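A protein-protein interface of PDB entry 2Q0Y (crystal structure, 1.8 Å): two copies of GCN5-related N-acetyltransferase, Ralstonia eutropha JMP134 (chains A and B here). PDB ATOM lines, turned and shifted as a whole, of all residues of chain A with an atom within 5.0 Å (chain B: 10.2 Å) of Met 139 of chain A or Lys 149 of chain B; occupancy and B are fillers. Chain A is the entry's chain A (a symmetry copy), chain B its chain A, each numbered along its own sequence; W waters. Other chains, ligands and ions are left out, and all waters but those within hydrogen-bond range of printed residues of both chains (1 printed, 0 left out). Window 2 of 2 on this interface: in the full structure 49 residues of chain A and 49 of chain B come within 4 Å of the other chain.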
ATOM      1  N   GLN A 106     -21.152  27.729   3.736  1.00  0.00           N
ATOM      2  CA  GLN A 106     -19.762  28.179   3.864  1.00  0.00           C
ATOM      3  C   GLN A 106     -19.515  28.889   5.196  1.00  0.00           C
ATOM      4  O   GLN A 106     -18.485  28.678   5.841  1.00  0.00           O
ATOM      5  CB  GLN A 106     -19.390  29.061   2.685  1.00  0.00           C
ATOM      6  CG  GLN A 106     -17.964  29.582   2.768  1.00  0.00           C
ATOM      7  CD  GLN A 106     -17.463  30.178   1.474  1.00  0.00           C
ATOM      8  OE1 GLN A 106     -18.229  30.404   0.541  1.00  0.00           O
ATOM      9  NE2 GLN A 106     -16.159  30.436   1.413  1.00  0.00           N
ATOM     10  N   MET A 109     -19.353  26.211   7.850  1.00  0.00           N
ATOM     11  CA  MET A 109     -18.060  25.546   7.731  1.00  0.00           C
ATOM     12  C   MET A 109     -16.941  26.411   8.302  1.00  0.00           C
ATOM     13  O   MET A 109     -16.048  25.906   8.979  1.00  0.00           O
ATOM     14  CB  MET A 109     -17.758  25.190   6.287  1.00  0.00           C
ATOM     15  CG  MET A 109     -18.559  24.020   5.738  1.00  0.00           C
ATOM     16  SD  MET A 109     -18.022  22.319   6.463  1.00  0.00           S
ATOM     17  CE  MET A 109     -16.196  22.213   5.760  1.00  0.00           C
ATOM     18  N   ASN A 110     -16.980  27.706   8.028  1.00  0.00           N
ATOM     19  CA  ASN A 110     -15.973  28.615   8.565  1.00  0.00           C
ATOM     20  C   ASN A 110     -15.987  28.622  10.081  1.00  0.00           C
ATOM     21  O   ASN A 110     -14.914  28.617  10.712  1.00  0.00           O
ATOM     22  CB  ASN A 110     -16.192  30.047   8.053  1.00  0.00           C
ATOM     23  CG  ASN A 110     -15.709  30.249   6.634  1.00  0.00           C
ATOM     24  OD1 ASN A 110     -14.829  29.554   6.155  1.00  0.00           O
ATOM     25  ND2 ASN A 110     -16.271  31.250   5.967  1.00  0.00           N
ATOM     26  N   GLU A 113     -14.452  25.210  11.268  1.00  0.00           N
ATOM     27  CA  GLU A 113     -12.997  25.207  11.106  1.00  0.00           C
ATOM     28  C   GLU A 113     -12.307  26.140  12.124  1.00  0.00           C
ATOM     29  O   GLU A 113     -11.268  25.792  12.678  1.00  0.00           O
ATOM     30  CB  GLU A 113     -12.595  25.586   9.696  1.00  0.00           C
ATOM     31  CG  GLU A 113     -13.044  24.553   8.658  1.00  0.00           C
ATOM     32  CD  GLU A 113     -12.702  24.938   7.229  1.00  0.00           C
ATOM     33  OE1 GLU A 113     -11.914  25.884   6.996  1.00  0.00           O
ATOM     34  OE2 GLU A 113     -13.281  24.301   6.333  1.00  0.00           O
ATOM     35  N   ALA A 122      -4.900  19.906  14.739  1.00  0.00           N
ATOM     36  CA  ALA A 122      -4.043  19.923  13.543  1.00  0.00           C
ATOM     37  C   ALA A 122      -4.764  19.585  12.233  1.00  0.00           C
ATOM     38  O   ALA A 122      -4.448  20.145  11.190  1.00  0.00           O
ATOM     39  CB  ALA A 122      -2.866  18.964  13.736  1.00  0.00           C
ATOM     40  N   PHE A 123      -5.727  18.671  12.290  1.00  0.00           N
ATOM     41  CA  PHE A 123      -6.246  18.021  11.076  1.00  0.00           C
ATOM     42  C   PHE A 123      -7.699  17.656  11.296  1.00  0.00           C
ATOM     43  O   PHE A 123      -8.070  17.249  12.400  1.00  0.00           O
ATOM     44  CB  PHE A 123      -5.398  16.766  10.826  1.00  0.00           C
ATOM     45  CG  PHE A 123      -5.648  16.070   9.518  1.00  0.00           C
ATOM     46  CD1 PHE A 123      -5.217  16.622   8.322  1.00  0.00           C
ATOM     47  CD2 PHE A 123      -6.265  14.827   9.494  1.00  0.00           C
ATOM     48  CE1 PHE A 123      -5.415  15.944   7.125  1.00  0.00           C
ATOM     49  CE2 PHE A 123      -6.446  14.151   8.289  1.00  0.00           C
ATOM     50  CZ  PHE A 123      -6.019  14.722   7.123  1.00  0.00           C
ATOM     51  N   ALA A 124      -8.510  17.783  10.251  1.00  0.00           N
ATOM     52  CA  ALA A 124      -9.927  17.444  10.332  1.00  0.00           C
ATOM     53  C   ALA A 124     -10.386  16.678   9.105  1.00  0.00           C
ATOM     54  O   ALA A 124      -9.773  16.774   8.015  1.00  0.00           O
ATOM     55  CB  ALA A 124     -10.744  18.712  10.483  1.00  0.00           C
ATOM     56  N   LEU A 135     -18.274  22.851  -2.702  1.00  0.00           N
ATOM     57  CA  LEU A 135     -17.977  23.849  -1.680  1.00  0.00           C
ATOM     58  C   LEU A 135     -16.752  23.436  -0.873  1.00  0.00           C
ATOM     59  O   LEU A 135     -15.857  24.237  -0.639  1.00  0.00           O
ATOM     60  CB  LEU A 135     -19.180  24.052  -0.743  1.00  0.00           C
ATOM     61  CG  LEU A 135     -18.928  24.902   0.511  1.00  0.00           C
ATOM     62  CD1 LEU A 135     -18.530  26.333   0.120  1.00  0.00           C
ATOM     63  CD2 LEU A 135     -20.136  24.882   1.431  1.00  0.00           C
ATOM     64  N   TYR A 136     -16.705  22.174  -0.452  1.00  0.00           N
ATOM     65  CA  TYR A 136     -15.592  21.745   0.386  1.00  0.00           C
ATOM     66  C   TYR A 136     -14.292  21.862  -0.398  1.00  0.00           C
ATOM     67  O   TYR A 136     -13.289  22.354   0.120  1.00  0.00           O
ATOM     68  CB  TYR A 136     -15.807  20.328   0.951  1.00  0.00           C
ATOM     69  CG  TYR A 136     -17.163  20.123   1.602  1.00  0.00           C
ATOM     70  CD1 TYR A 136     -17.784  21.148   2.339  1.00  0.00           C
ATOM     71  CD2 TYR A 136     -17.849  18.919   1.456  1.00  0.00           C
ATOM     72  CE1 TYR A 136     -19.031  20.959   2.915  1.00  0.00           C
ATOM     73  CE2 TYR A 136     -19.093  18.725   2.026  1.00  0.00           C
ATOM     74  CZ  TYR A 136     -19.682  19.740   2.760  1.00  0.00           C
ATOM     75  OH  TYR A 136     -20.933  19.543   3.310  1.00  0.00           O
ATOM     76  N   ALA A 137     -14.314  21.436  -1.653  1.00  0.00           N
ATOM     77  CA  ALA A 137     -13.131  21.530  -2.488  1.00  0.00           C
ATOM     78  C   ALA A 137     -12.697  22.982  -2.627  1.00  0.00           C
ATOM     79  O   ALA A 137     -11.506  23.274  -2.526  1.00  0.00           O
ATOM     80  CB  ALA A 137     -13.386  20.926  -3.826  1.00  0.00           C
ATOM     81  N   ARG A 138     -13.651  23.882  -2.856  1.00  0.00           N
ATOM     82  CA  ARG A 138     -13.366  25.322  -2.929  1.00  0.00           C
ATOM     83  C   ARG A 138     -12.715  25.823  -1.648  1.00  0.00           C
ATOM     84  O   ARG A 138     -11.872  26.726  -1.676  1.00  0.00           O
ATOM     85  CB  ARG A 138     -14.648  26.137  -3.160  1.00  0.00           C
ATOM     86  CG  ARG A 138     -15.181  26.112  -4.575  1.00  0.00           C
ATOM     87  CD  ARG A 138     -16.277  27.169  -4.797  1.00  0.00           C
ATOM     88  NE  ARG A 138     -17.595  26.748  -4.309  1.00  0.00           N
ATOM     89  CZ  ARG A 138     -18.283  27.321  -3.316  1.00  0.00           C
ATOM     90  NH1 ARG A 138     -17.806  28.378  -2.650  1.00  0.00           N
ATOM     91  NH2 ARG A 138     -19.478  26.830  -2.990  1.00  0.00           N
ATOM     92  N   MET A 139     -13.129  25.247  -0.524  1.00  0.00           N
ATOM     93  CA  MET A 139     -12.633  25.647   0.782  1.00  0.00           C
ATOM     94  C   MET A 139     -11.361  24.896   1.209  1.00  0.00           C
ATOM     95  O   MET A 139     -10.953  24.996   2.365  1.00  0.00           O
ATOM     96  CB  MET A 139     -13.725  25.455   1.820  1.00  0.00           C
ATOM     97  CG  MET A 139     -14.964  26.338   1.623  1.00  0.00           C
ATOM     98  SD  MET A 139     -16.191  26.051   3.116  1.00  0.00           S
ATOM     99  CE  MET A 139     -15.054  26.814   4.521  1.00  0.00           C
ATOM    100  N   GLY A 140     -10.741  24.161   0.283  1.00  0.00           N
ATOM    101  CA  GLY A 140      -9.423  23.573   0.521  1.00  0.00           C
ATOM    102  C   GLY A 140      -9.428  22.183   1.116  1.00  0.00           C
ATOM    103  O   GLY A 140      -8.405  21.712   1.643  1.00  0.00           O
ATOM    104  N   TRP A 141     -10.582  21.517   1.036  1.00  0.00           N
ATOM    105  CA  TRP A 141     -10.715  20.128   1.454  1.00  0.00           C
ATOM    106  C   TRP A 141     -10.299  19.208   0.295  1.00  0.00           C
ATOM    107  O   TRP A 141     -10.529  19.524  -0.885  1.00  0.00           O
ATOM    108  CB  TRP A 141     -12.136  19.811   1.922  1.00  0.00           C
ATOM    109  CG  TRP A 141     -12.504  20.546   3.181  1.00  0.00           C
ATOM    110  CD1 TRP A 141     -12.841  21.860   3.296  1.00  0.00           C
ATOM    111  CD2 TRP A 141     -12.559  19.998   4.498  1.00  0.00           C
ATOM    112  NE1 TRP A 141     -13.095  22.167   4.613  1.00  0.00           N
ATOM    113  CE2 TRP A 141     -12.901  21.043   5.375  1.00  0.00           C
ATOM    114  CE3 TRP A 141     -12.308  18.717   5.033  1.00  0.00           C
ATOM    115  CZ2 TRP A 141     -13.038  20.846   6.752  1.00  0.00           C
ATOM    116  CZ3 TRP A 141     -12.437  18.530   6.383  1.00  0.00           C
ATOM    117  CH2 TRP A 141     -12.797  19.584   7.234  1.00  0.00           C
ATOM    118  N   GLU B 146     -15.044  10.600   2.096  1.00  0.00           N
ATOM    119  CA  GLU B 146     -14.263  11.341   3.071  1.00  0.00           C
ATOM    120  C   GLU B 146     -13.360  12.368   2.409  1.00  0.00           C
ATOM    121  O   GLU B 146     -12.756  12.119   1.360  1.00  0.00           O
ATOM    122  CB  GLU B 146     -13.438  10.390   3.934  1.00  0.00           C
ATOM    123  CG  GLU B 146     -12.792  11.087   5.111  1.00  0.00           C
ATOM    124  CD  GLU B 146     -11.948  10.170   5.939  1.00  0.00           C
ATOM    125  OE1 GLU B 146     -10.894   9.712   5.476  1.00  0.00           O
ATOM    126  OE2 GLU B 146     -12.359   9.902   7.070  1.00  0.00           O
ATOM    127  N   MET B 147     -13.281  13.532   3.044  1.00  0.00           N
ATOM    128  CA  MET B 147     -12.373  14.579   2.654  1.00  0.00           C
ATOM    129  C   MET B 147     -11.696  15.095   3.912  1.00  0.00           C
ATOM    130  O   MET B 147     -12.205  14.919   5.021  1.00  0.00           O
ATOM    131  CB  MET B 147     -13.125  15.720   1.945  1.00  0.00           C
ATOM    132  CG  MET B 147     -13.933  15.266   0.730  1.00  0.00           C
ATOM    133  SD  MET B 147     -14.892  16.696  -0.104  1.00  0.00           S
ATOM    134  CE  MET B 147     -13.431  17.531  -1.007  1.00  0.00           C
ATOM    135  N   SER B 148     -10.555  15.744   3.727  1.00  0.00           N
ATOM    136  CA  SER B 148      -9.747  16.214   4.834  1.00  0.00           C
ATOM    137  C   SER B 148      -9.178  17.602   4.578  1.00  0.00           C
ATOM    138  O   SER B 148      -9.097  18.059   3.427  1.00  0.00           O
ATOM    139  CB  SER B 148      -8.607  15.229   5.110  1.00  0.00           C
ATOM    140  OG  SER B 148      -7.613  15.243   4.077  1.00  0.00           O
ATOM    141  N   LYS B 149      -8.777  18.262   5.668  1.00  0.00           N
ATOM    142  CA  LYS B 149      -8.156  19.562   5.606  1.00  0.00           C
ATOM    143  C   LYS B 149      -7.254  19.807   6.825  1.00  0.00           C
ATOM    144  O   LYS B 149      -7.666  19.558   7.961  1.00  0.00           O
ATOM    145  CB  LYS B 149      -9.217  20.656   5.534  1.00  0.00           C
ATOM    146  CG  LYS B 149      -8.662  22.044   5.384  1.00  0.00           C
ATOM    147  CD  LYS B 149      -9.742  23.099   5.305  1.00  0.00           C
ATOM    148  CE  LYS B 149      -9.149  24.465   5.108  1.00  0.00           C
ATOM    149  NZ  LYS B 149     -10.198  25.529   4.953  1.00  0.00           N
ATOM    150  N   PRO B 150      -6.015  20.265   6.598  1.00  0.00           N
ATOM    151  CA  PRO B 150      -5.227  20.703   7.735  1.00  0.00           C
ATOM    152  C   PRO B 150      -5.857  21.947   8.333  1.00  0.00           C
ATOM    153  O   PRO B 150      -6.332  22.816   7.598  1.00  0.00           O
ATOM    154  CB  PRO B 150      -3.872  21.044   7.115  1.00  0.00           C
ATOM    155  CG  PRO B 150      -3.860  20.253   5.830  1.00  0.00           C
ATOM    156  CD  PRO B 150      -5.239  20.354   5.344  1.00  0.00           C
ATOM    157  N   ILE B 151      -5.859  22.025   9.656  1.00  0.00           N
ATOM    158  CA  ILE B 151      -6.414  23.193  10.351  1.00  0.00           C
ATOM    159  C   ILE B 151      -5.242  23.974  10.946  1.00  0.00           C
ATOM    160  O   ILE B 151      -4.773  24.927  10.327  1.00  0.00           O
ATOM    161  CB  ILE B 151      -7.445  22.774  11.415  1.00  0.00           C
ATOM    162  CG1 ILE B 151      -8.536  21.902  10.803  1.00  0.00           C
ATOM    163  CG2 ILE B 151      -8.038  24.004  12.094  1.00  0.00           C
ATOM    164  CD1 ILE B 151      -9.392  22.587   9.741  1.00  0.00           C
ATOM    165  N   ALA B 152      -4.758  23.586  12.123  1.00  0.00           N
ATOM    166  CA  ALA B 152      -3.581  24.234  12.715  1.00  0.00           C
ATOM    167  C   ALA B 152      -2.276  23.579  12.224  1.00  0.00           C
ATOM    168  O   ALA B 152      -1.202  24.163  12.331  1.00  0.00           O
ATOM    169  CB  ALA B 152      -3.668  24.199  14.233  1.00  0.00           C
ATOM    170  N   GLY B 153      -2.395  22.372  11.659  1.00  0.00           N
ATOM    171  CA  GLY B 153      -1.259  21.607  11.140  1.00  0.00           C
ATOM    172  C   GLY B 153      -1.046  21.808   9.647  1.00  0.00           C
ATOM    173  O   GLY B 153      -1.277  22.894   9.085  1.00  0.00           O
ATOM    174  OXT GLY B 153      -0.615  20.868   8.956  1.00  0.00           O
HETATM  175  O   HOH W   1      -6.666  19.543   1.826  1.00  0.00           O
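The side-chain carboxylate (OE1) of Glu 113 of chain A lies within salt-bridge range of the side-chain amino group (NZ) of Lys 149 of chain B, 2.7 Å away. The backbone NH (N) of Lys 149 of chain B is in hydrogen-bond range of the backbone carbonyl oxygen (O) of Ala 124 of chain A. NZ of Lys 149 of chain B is in hydrogen-bond range of O of Met 139 of chain A. The backbone carbonyl oxygen (O) of Ala 122 of chain A sits at hydrogen-bond distance from the backbone NH (N) of Ile 151 of chain B. The backbone NH (N) of Gly 153 of chain B lies within hydrogen-bond range of the backbone carbonyl oxygen (O) of Ala 122 of chain A (3.1 Å).
NE1 of Trp 141 of chain A is in hydrogen-bond range of OE2 of Glu 113 of chain A (2.7 Å). The backbone carbonyl oxygen (O) of Tyr 136 of chain A lies within hydrogen-bond range of the backbone NH (N) of Trp 141 of chain A, 3.0 Å away.
Among the printed residues, pairs that only touch across the chains: Ala 124 of chain A with Ser 148 of chain B, Trp 141 of chain A with Ser 148 of chain B, Phe 123 of chain A with Ser 148 of chain B, Trp 141 of chain A with Met 147 of chain B, Trp 141 of chain A with Lys 149 of chain B, Ala 122 of chain A with Ala 152 of chain B, Ala 122 of chain A with Pro 150 of chain B, Glu 113 of chain A with Ile 151 of chain B, Phe 123 of chain A with Lys 149 of chain B, Gly 140 of chain A with Lys 149 of chain B, Tyr 136 of chain A with Met 147 of chain B and Ala 124 of chain A with Ile 151 of chain B.
Of chain B, only Lys 149 (2.7 Å) comes within 4 Å of Met 139 of chain A. Printed residues of chain A within 4 Å of Lys 149 of chain B: Glu 113 (2.7 Å), Phe 123 (3.8 Å), Ala 124 (3.0 Å), Met 139 (2.7 Å), Gly 140 (3.8 Å) and Trp 141 (3.5 Å). No residue of chain B comes within 4 Å of Met 109 of chain A. Phe 123 of chain A touches two residues of chain B. Ala 124 of chain A touches just these residues of chain B: Ser 148 (3.2 Å), Lys 149 (3.0 Å) and Ile 151 (3.9 Å). No residue of chain B comes within 4 Å of Leu 135 of chain A. No residue of chain B comes within 4 Å of Ala 137 of chain A. Gly 140 of chain A touches just one residue of chain B: Lys 149 (3.8 Å). Of the printed residues of chain A, Ser 148 of chain B touches Phe 123, Ala 124 and Trp 141. Printed residues of chain B within 4 Å of Tyr 136 of chain A: Met 147. Of the printed residues of chain B, Ala 122 of chain A touches Pro 150, Ile 151, Ala 152 and Gly 153. Printed residues of chain A within 4 Å of Ala 152 of chain B: Ala 122. Asn 110 of chain A touches none of the printed residues of chain B. Glu 146 of chain B touches none of the printed residues of chain A. The nearest residue of chain B that does not touch Met 139 of chain A is Ser 148 of chain B (7.3 Å). The nearest residue of chain A that does not touch Lys 149 of chain B is Ala 122 of chain A (4.6 Å). The nearest printed residue of chain A that does not touch Gly 153 of chain B is Phe 123 of chain A (5.0 Å).
Of the 8 printed residues of chain B, 7 touch a printed residue of chain A. Of the 14 printed residues of chain A, 8 touch a printed residue of chain B.
No position is printed for both chains.
Water W1 bridges O of Gly 140 of chain A (2.8 Å) and O of Ser 148 of chain B (3.3 Å).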
